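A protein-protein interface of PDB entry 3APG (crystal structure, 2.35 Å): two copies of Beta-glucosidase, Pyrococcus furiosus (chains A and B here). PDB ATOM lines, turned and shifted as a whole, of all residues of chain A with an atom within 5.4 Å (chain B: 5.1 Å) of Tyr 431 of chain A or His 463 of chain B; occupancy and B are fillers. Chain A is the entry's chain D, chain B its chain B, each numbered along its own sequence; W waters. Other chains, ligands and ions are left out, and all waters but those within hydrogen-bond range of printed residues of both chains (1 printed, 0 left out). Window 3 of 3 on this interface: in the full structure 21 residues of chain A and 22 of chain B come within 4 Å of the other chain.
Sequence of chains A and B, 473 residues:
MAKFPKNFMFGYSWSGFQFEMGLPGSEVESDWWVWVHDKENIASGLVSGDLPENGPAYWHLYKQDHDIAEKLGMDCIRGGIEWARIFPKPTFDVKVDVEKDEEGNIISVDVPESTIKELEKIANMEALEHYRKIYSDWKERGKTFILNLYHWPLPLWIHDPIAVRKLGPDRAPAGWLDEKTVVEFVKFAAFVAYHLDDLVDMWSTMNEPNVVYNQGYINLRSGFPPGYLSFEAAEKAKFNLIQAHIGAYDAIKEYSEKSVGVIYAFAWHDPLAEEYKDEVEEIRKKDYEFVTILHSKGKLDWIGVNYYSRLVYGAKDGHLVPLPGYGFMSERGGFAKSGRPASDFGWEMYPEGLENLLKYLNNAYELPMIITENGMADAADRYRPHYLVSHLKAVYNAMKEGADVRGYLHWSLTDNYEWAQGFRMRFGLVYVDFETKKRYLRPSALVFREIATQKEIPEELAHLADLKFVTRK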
ATOM      1  N   ASP A 415      18.660 -14.468   2.474  1.00  0.00           N
ATOM      2  CA  ASP A 415      17.467 -15.103   1.923  1.00  0.00           C
ATOM      3  C   ASP A 415      17.435 -14.782   0.424  1.00  0.00           C
ATOM      4  O   ASP A 415      18.006 -13.772   0.014  1.00  0.00           O
ATOM      5  CB  ASP A 415      16.174 -14.526   2.579  1.00  0.00           C
ATOM      6  CG  ASP A 415      16.097 -14.795   4.095  1.00  0.00           C
ATOM      7  OD1 ASP A 415      16.819 -15.727   4.577  1.00  0.00           O
ATOM      8  OD2 ASP A 415      15.325 -14.063   4.783  1.00  0.00           O
ATOM      9  N   ARG A 426      13.659 -19.612   3.561  1.00  0.00           N
ATOM     10  CA  ARG A 426      14.636 -18.572   3.879  1.00  0.00           C
ATOM     11  C   ARG A 426      15.931 -19.179   4.436  1.00  0.00           C
ATOM     12  O   ARG A 426      15.940 -19.660   5.559  1.00  0.00           O
ATOM     13  CB  ARG A 426      14.043 -17.548   4.850  1.00  0.00           C
ATOM     14  CG  ARG A 426      12.939 -16.684   4.203  1.00  0.00           C
ATOM     15  CD  ARG A 426      12.250 -15.699   5.206  1.00  0.00           C
ATOM     16  NE  ARG A 426      11.304 -14.828   4.483  1.00  0.00           N
ATOM     17  CZ  ARG A 426      11.645 -13.699   3.855  1.00  0.00           C
ATOM     18  NH1 ARG A 426      12.927 -13.299   3.862  1.00  0.00           N
ATOM     19  NH2 ARG A 426      10.719 -12.978   3.197  1.00  0.00           N
ATOM     20  N   GLY A 428      19.116 -17.537   4.527  1.00  0.00           N
ATOM     21  CA  GLY A 428      20.154 -16.570   4.843  1.00  0.00           C
ATOM     22  C   GLY A 428      20.654 -16.523   6.292  1.00  0.00           C
ATOM     23  O   GLY A 428      19.879 -16.689   7.238  1.00  0.00           O
ATOM     24  N   LEU A 429      21.970 -16.243   6.426  1.00  0.00           N
ATOM     25  CA  LEU A 429      22.547 -15.716   7.641  1.00  0.00           C
ATOM     26  C   LEU A 429      21.966 -14.336   7.868  1.00  0.00           C
ATOM     27  O   LEU A 429      22.027 -13.811   8.995  1.00  0.00           O
ATOM     28  CB  LEU A 429      24.037 -15.606   7.468  1.00  0.00           C
ATOM     29  CG  LEU A 429      24.793 -16.931   7.459  1.00  0.00           C
ATOM     30  CD1 LEU A 429      26.276 -16.661   7.311  1.00  0.00           C
ATOM     31  CD2 LEU A 429      24.498 -17.648   8.744  1.00  0.00           C
ATOM     32  N   VAL A 430      21.391 -13.764   6.800  1.00  0.00           N
ATOM     33  CA  VAL A 430      20.905 -12.391   6.778  1.00  0.00           C
ATOM     34  C   VAL A 430      19.470 -12.351   6.182  1.00  0.00           C
ATOM     35  O   VAL A 430      19.242 -12.751   5.023  1.00  0.00           O
ATOM     36  CB  VAL A 430      21.833 -11.455   5.941  1.00  0.00           C
ATOM     37  CG1 VAL A 430      21.161 -10.076   5.738  1.00  0.00           C
ATOM     38  CG2 VAL A 430      23.310 -11.338   6.498  1.00  0.00           C
ATOM     39  N   TYR A 431      18.507 -11.911   6.972  1.00  0.00           N
ATOM     40  CA  TYR A 431      17.150 -11.795   6.512  1.00  0.00           C
ATOM     41  C   TYR A 431      16.993 -10.678   5.457  1.00  0.00           C
ATOM     42  O   TYR A 431      17.580  -9.582   5.606  1.00  0.00           O
ATOM     43  CB  TYR A 431      16.250 -11.469   7.718  1.00  0.00           C
ATOM     44  CG  TYR A 431      14.873 -10.906   7.352  1.00  0.00           C
ATOM     45  CD1 TYR A 431      14.484  -9.632   7.778  1.00  0.00           C
ATOM     46  CD2 TYR A 431      13.954 -11.655   6.578  1.00  0.00           C
ATOM     47  CE1 TYR A 431      13.210  -9.112   7.448  1.00  0.00           C
ATOM     48  CE2 TYR A 431      12.694 -11.137   6.262  1.00  0.00           C
ATOM     49  CZ  TYR A 431      12.338  -9.874   6.705  1.00  0.00           C
ATOM     50  OH  TYR A 431      11.126  -9.364   6.382  1.00  0.00           O
ATOM     51  N   VAL A 432      16.177 -10.910   4.430  1.00  0.00           N
ATOM     52  CA  VAL A 432      15.880  -9.831   3.471  1.00  0.00           C
ATOM     53  C   VAL A 432      14.390  -9.628   3.417  1.00  0.00           C
ATOM     54  O   VAL A 432      13.664 -10.571   3.072  1.00  0.00           O
ATOM     55  CB  VAL A 432      16.343 -10.153   2.043  1.00  0.00           C
ATOM     56  CG1 VAL A 432      15.914  -9.027   1.100  1.00  0.00           C
ATOM     57  CG2 VAL A 432      17.871 -10.339   2.001  1.00  0.00           C
ATOM     58  N   ASP A 433      13.933  -8.415   3.798  1.00  0.00           N
ATOM     59  CA  ASP A 433      12.616  -7.934   3.499  1.00  0.00           C
ATOM     60  C   ASP A 433      12.520  -7.678   1.990  1.00  0.00           C
ATOM     61  O   ASP A 433      13.117  -6.710   1.453  1.00  0.00           O
ATOM     62  CB  ASP A 433      12.352  -6.637   4.232  1.00  0.00           C
ATOM     63  CG  ASP A 433      10.956  -6.063   3.911  1.00  0.00           C
ATOM     64  OD1 ASP A 433      10.417  -6.267   2.791  1.00  0.00           O
ATOM     65  OD2 ASP A 433      10.366  -5.407   4.781  1.00  0.00           O
ATOM     66  N   PHE A 434      11.744  -8.492   1.293  1.00  0.00           N
ATOM     67  CA  PHE A 434      11.746  -8.363  -0.171  1.00  0.00           C
ATOM     68  C   PHE A 434      10.956  -7.172  -0.701  1.00  0.00           C
ATOM     69  O   PHE A 434      10.963  -6.901  -1.896  1.00  0.00           O
ATOM     70  CB  PHE A 434      11.350  -9.658  -0.856  1.00  0.00           C
ATOM     71  CG  PHE A 434      12.313 -10.798  -0.619  1.00  0.00           C
ATOM     72  CD1 PHE A 434      13.550 -10.835  -1.250  1.00  0.00           C
ATOM     73  CD2 PHE A 434      11.970 -11.855   0.206  1.00  0.00           C
ATOM     74  CE1 PHE A 434      14.421 -11.908  -1.063  1.00  0.00           C
ATOM     75  CE2 PHE A 434      12.843 -12.930   0.437  1.00  0.00           C
ATOM     76  CZ  PHE A 434      14.074 -12.937  -0.184  1.00  0.00           C
ATOM     77  N   LYS A 438      15.670  -4.170   2.275  1.00  0.00           N
ATOM     78  CA  LYS A 438      16.514  -4.070   3.481  1.00  0.00           C
ATOM     79  C   LYS A 438      17.042  -5.429   4.033  1.00  0.00           C
ATOM     80  O   LYS A 438      16.311  -6.439   4.052  1.00  0.00           O
ATOM     81  CB  LYS A 438      15.847  -3.238   4.571  1.00  0.00           C
ATOM     82  CG  LYS A 438      16.036  -1.808   4.288  1.00  0.00           C
ATOM     83  CD  LYS A 438      15.116  -0.849   5.154  1.00  0.00           C
ATOM     84  CE  LYS A 438      15.345   0.644   4.730  1.00  0.00           C
ATOM     85  NZ  LYS A 438      15.235   1.620   5.865  1.00  0.00           N
ATOM     86  N   ARG A 439      18.311  -5.416   4.462  1.00  0.00           N
ATOM     87  CA  ARG A 439      18.972  -6.598   5.068  1.00  0.00           C
ATOM     88  C   ARG A 439      18.983  -6.553   6.593  1.00  0.00           C
ATOM     89  O   ARG A 439      19.290  -5.512   7.195  1.00  0.00           O
ATOM     90  CB  ARG A 439      20.411  -6.719   4.598  1.00  0.00           C
ATOM     91  CG  ARG A 439      20.645  -7.375   3.184  1.00  0.00           C
ATOM     92  CD  ARG A 439      20.242  -6.468   2.018  1.00  0.00           C
ATOM     93  NE  ARG A 439      20.694  -7.095   0.770  1.00  0.00           N
ATOM     94  CZ  ARG A 439      19.944  -7.267  -0.307  1.00  0.00           C
ATOM     95  NH1 ARG A 439      18.694  -6.850  -0.339  1.00  0.00           N
ATOM     96  NH2 ARG A 439      20.455  -7.853  -1.376  1.00  0.00           N
ATOM     97  N   TYR A 440      18.696  -7.676   7.250  1.00  0.00           N
ATOM     98  CA  TYR A 440      18.940  -7.678   8.700  1.00  0.00           C
ATOM     99  C   TYR A 440      19.754  -8.842   9.104  1.00  0.00           C
ATOM    100  O   TYR A 440      19.643  -9.902   8.505  1.00  0.00           O
ATOM    101  CB  TYR A 440      17.643  -7.705   9.449  1.00  0.00           C
ATOM    102  CG  TYR A 440      16.740  -6.624   9.032  1.00  0.00           C
ATOM    103  CD1 TYR A 440      16.498  -5.566   9.885  1.00  0.00           C
ATOM    104  CD2 TYR A 440      16.127  -6.635   7.764  1.00  0.00           C
ATOM    105  CE1 TYR A 440      15.614  -4.527   9.533  1.00  0.00           C
ATOM    106  CE2 TYR A 440      15.250  -5.597   7.379  1.00  0.00           C
ATOM    107  CZ  TYR A 440      14.986  -4.573   8.279  1.00  0.00           C
ATOM    108  OH  TYR A 440      14.156  -3.544   7.959  1.00  0.00           O
ATOM    109  N   LEU A 441      20.602  -8.658  10.114  1.00  0.00           N
ATOM    110  CA  LEU A 441      21.425  -9.768  10.619  1.00  0.00           C
ATOM    111  C   LEU A 441      20.571 -10.737  11.396  1.00  0.00           C
ATOM    112  O   LEU A 441      19.616 -10.325  12.089  1.00  0.00           O
ATOM    113  CB  LEU A 441      22.517  -9.242  11.528  1.00  0.00           C
ATOM    114  CG  LEU A 441      23.654  -8.533  10.796  1.00  0.00           C
ATOM    115  CD1 LEU A 441      24.810  -8.299  11.746  1.00  0.00           C
ATOM    116  CD2 LEU A 441      24.140  -9.307   9.574  1.00  0.00           C
ATOM    117  N   ARG A 442      20.864 -12.016  11.265  1.00  0.00           N
ATOM    118  CA  ARG A 442      20.324 -13.023  12.160  1.00  0.00           C
ATOM    119  C   ARG A 442      21.484 -13.364  13.118  1.00  0.00           C
ATOM    120  O   ARG A 442      22.652 -13.254  12.727  1.00  0.00           O
ATOM    121  CB  ARG A 442      19.894 -14.250  11.387  1.00  0.00           C
ATOM    122  CG  ARG A 442      18.637 -14.048  10.441  1.00  0.00           C
ATOM    123  CD  ARG A 442      17.996 -15.381   9.950  1.00  0.00           C
ATOM    124  NE  ARG A 442      16.723 -15.156   9.259  1.00  0.00           N
ATOM    125  CZ  ARG A 442      16.542 -15.254   7.931  1.00  0.00           C
ATOM    126  NH1 ARG A 442      17.524 -15.686   7.110  1.00  0.00           N
ATOM    127  NH2 ARG A 442      15.362 -14.966   7.430  1.00  0.00           N
ATOM    128  N   HIS B 386      14.604 -13.738  19.755  1.00  0.00           N
ATOM    129  CA  HIS B 386      13.349 -13.001  19.533  1.00  0.00           C
ATOM    130  C   HIS B 386      12.690 -12.535  20.826  1.00  0.00           C
ATOM    131  O   HIS B 386      12.166 -11.412  20.879  1.00  0.00           O
ATOM    132  CB  HIS B 386      12.357 -13.795  18.690  1.00  0.00           C
ATOM    133  CG  HIS B 386      12.638 -13.764  17.216  1.00  0.00           C
ATOM    134  ND1 HIS B 386      13.510 -14.646  16.603  1.00  0.00           N
ATOM    135  CD2 HIS B 386      12.138 -12.993  16.216  1.00  0.00           C
ATOM    136  CE1 HIS B 386      13.535 -14.419  15.297  1.00  0.00           C
ATOM    137  NE2 HIS B 386      12.718 -13.425  15.032  1.00  0.00           N
ATOM    138  N   GLU B 459      19.503  -0.903  13.984  1.00  0.00           N
ATOM    139  CA  GLU B 459      18.800  -1.253  12.768  1.00  0.00           C
ATOM    140  C   GLU B 459      18.993  -2.733  12.312  1.00  0.00           C
ATOM    141  O   GLU B 459      18.018  -3.428  12.001  1.00  0.00           O
ATOM    142  CB  GLU B 459      19.319  -0.336  11.690  1.00  0.00           C
ATOM    143  CG  GLU B 459      18.269   0.447  10.918  1.00  0.00           C
ATOM    144  CD  GLU B 459      17.192  -0.441  10.289  1.00  0.00           C
ATOM    145  OE1 GLU B 459      17.226  -0.624   9.013  1.00  0.00           O
ATOM    146  OE2 GLU B 459      16.304  -0.913  11.081  1.00  0.00           O
ATOM    147  N   LEU B 461      19.519  -5.250  13.943  1.00  0.00           N
ATOM    148  CA  LEU B 461      18.867  -6.233  14.812  1.00  0.00           C
ATOM    149  C   LEU B 461      17.351  -5.960  15.047  1.00  0.00           C
ATOM    150  O   LEU B 461      16.690  -6.693  15.783  1.00  0.00           O
ATOM    151  CB  LEU B 461      19.608  -6.428  16.159  1.00  0.00           C
ATOM    152  CG  LEU B 461      21.096  -6.799  16.140  1.00  0.00           C
ATOM    153  CD1 LEU B 461      21.557  -6.954  17.533  1.00  0.00           C
ATOM    154  CD2 LEU B 461      21.413  -8.084  15.421  1.00  0.00           C
ATOM    155  N   ALA B 462      16.797  -4.954  14.381  1.00  0.00           N
ATOM    156  CA  ALA B 462      15.414  -4.553  14.618  1.00  0.00           C
ATOM    157  C   ALA B 462      14.433  -5.661  14.285  1.00  0.00           C
ATOM    158  O   ALA B 462      13.368  -5.743  14.886  1.00  0.00           O
ATOM    159  CB  ALA B 462      15.084  -3.266  13.836  1.00  0.00           C
ATOM    160  N   HIS B 463      14.777  -6.531  13.339  1.00  0.00           N
ATOM    161  CA  HIS B 463      13.860  -7.581  12.946  1.00  0.00           C
ATOM    162  C   HIS B 463      13.637  -8.712  13.953  1.00  0.00           C
ATOM    163  O   HIS B 463      12.655  -9.441  13.861  1.00  0.00           O
ATOM    164  CB  HIS B 463      14.276  -8.189  11.627  1.00  0.00           C
ATOM    165  CG  HIS B 463      13.182  -9.002  10.996  1.00  0.00           C
ATOM    166  ND1 HIS B 463      13.309 -10.363  10.731  1.00  0.00           N
ATOM    167  CD2 HIS B 463      11.931  -8.643  10.608  1.00  0.00           C
ATOM    168  CE1 HIS B 463      12.172 -10.799  10.225  1.00  0.00           C
ATOM    169  NE2 HIS B 463      11.325  -9.778  10.133  1.00  0.00           N
ATOM    170  N   LEU B 464      14.558  -8.877  14.897  1.00  0.00           N
ATOM    171  CA  LEU B 464      14.353  -9.786  16.013  1.00  0.00           C
ATOM    172  C   LEU B 464      13.194  -9.420  16.942  1.00  0.00           C
ATOM    173  O   LEU B 464      12.844 -10.190  17.833  1.00  0.00           O
ATOM    174  CB  LEU B 464      15.648  -9.831  16.843  1.00  0.00           C
ATOM    175  CG  LEU B 464      16.680 -10.703  16.138  1.00  0.00           C
ATOM    176  CD1 LEU B 464      18.061 -10.614  16.750  1.00  0.00           C
ATOM    177  CD2 LEU B 464      16.156 -12.079  16.252  1.00  0.00           C
ATOM    178  N   ALA B 465      12.673  -8.205  16.822  1.00  0.00           N
ATOM    179  CA  ALA B 465      11.541  -7.732  17.606  1.00  0.00           C
ATOM    180  C   ALA B 465      10.223  -8.164  16.971  1.00  0.00           C
ATOM    181  O   ALA B 465       9.204  -8.184  17.645  1.00  0.00           O
ATOM    182  CB  ALA B 465      11.587  -6.224  17.649  1.00  0.00           C
ATOM    183  N   ASP B 466      10.253  -8.481  15.657  1.00  0.00           N
ATOM    184  CA  ASP B 466       9.076  -8.908  14.895  1.00  0.00           C
ATOM    185  C   ASP B 466       8.828 -10.385  15.077  1.00  0.00           C
ATOM    186  O   ASP B 466       9.672 -11.183  14.720  1.00  0.00           O
ATOM    187  CB  ASP B 466       9.315  -8.628  13.418  1.00  0.00           C
ATOM    188  CG  ASP B 466       8.059  -8.770  12.576  1.00  0.00           C
ATOM    189  OD1 ASP B 466       7.042  -9.321  13.024  1.00  0.00           O
ATOM    190  OD2 ASP B 466       8.067  -8.331  11.415  1.00  0.00           O
ATOM    191  N   PHE B 469       7.739 -14.374  11.977  1.00  0.00           N
ATOM    192  CA  PHE B 469       8.328 -15.607  11.493  1.00  0.00           C
ATOM    193  C   PHE B 469       8.391 -16.675  12.540  1.00  0.00           C
ATOM    194  O   PHE B 469       8.615 -17.844  12.254  1.00  0.00           O
ATOM    195  CB  PHE B 469       9.725 -15.356  10.981  1.00  0.00           C
ATOM    196  CG  PHE B 469       9.732 -14.748   9.654  1.00  0.00           C
ATOM    197  CD1 PHE B 469       8.959 -15.284   8.631  1.00  0.00           C
ATOM    198  CD2 PHE B 469      10.452 -13.617   9.403  1.00  0.00           C
ATOM    199  CE1 PHE B 469       8.910 -14.682   7.378  1.00  0.00           C
ATOM    200  CE2 PHE B 469      10.407 -13.035   8.113  1.00  0.00           C
ATOM    201  CZ  PHE B 469       9.642 -13.571   7.124  1.00  0.00           C
HETATM  202  O   HOH W   1      17.127  -8.208  12.527  1.00  0.00           O
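Hydrophobic or aromatic side chains of chain B within 4 Å of the printed part of chain A: His 463 and Phe 469.
Printed residues of chain A that touch a printed residue of chain B: Arg 426, Tyr 431 and Tyr 440.
Hydrophobic or aromatic side chains of chain A within 4 Å of the printed part of chain B: Tyr 431 and Tyr 440.
Among the printed residues, no Asp or Glu carboxylate lies within 4 Å of a Lys or Arg side-chain nitrogen of the other chain.
No position is printed for both chains.
Of the 5 pairs that touch across the chains among the printed residues, none has its exchanged pair printed and touching as well.
Of the printed residues of chain B, Arg 426 of chain A touches Phe 469.
Tyr 431 of chain A touches just these residues of chain B: His 463 and Phe 469.
Lys 438 of chain A touches none of the printed residues of chain B.
Of the printed residues of chain B, Tyr 440 of chain A touches Glu 459 and His 463.
Printed residues of chain A within 4 Å of Glu 459 of chain B: Tyr 440 (3.4 Å).
His 463 of chain B touches two residues of chain A.
Printed residues of chain A within 4 Å of Phe 469 of chain B: Arg 426 and Tyr 431.
The nearest printed residue of chain B that does not touch Tyr 431 of chain A is Asp 466 of chain B (6.0 Å).
The side-chain carboxylate of Asp 415 of chain A is in salt-bridge range of the guanidinium group of Arg 426 of chain A, at 2.7 Å.
The guanidinium group of Arg 426 of chain A sits at hydrogen-bond distance from the backbone carbonyl oxygen of Val 432 of chain A, 2.9 Å away.
The backbone carbonyl oxygen (O) of Tyr 431 of chain A is in hydrogen-bond range of the backbone NH (N) of Tyr 440 of chain A, 2.8 Å away.
Water W1 lies within hydrogen-bond range of the backbone NH (N) of His 463 of chain B and the backbone carbonyl oxygen (O) of Leu 441 of chain A.
Among the printed residues, pairs that only touch across the chains: Tyr 431 of chain A with His 463 of chain B (3.3 Å), Arg 426 of chain A with Phe 469 of chain B (3.4 Å), Tyr 440 of chain A with Glu 459 of chain B (3.4 Å), Tyr 431 of chain A with Phe 469 of chain B (3.5 Å) and Tyr 440 of chain A with His 463 of chain B (3.9 Å).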
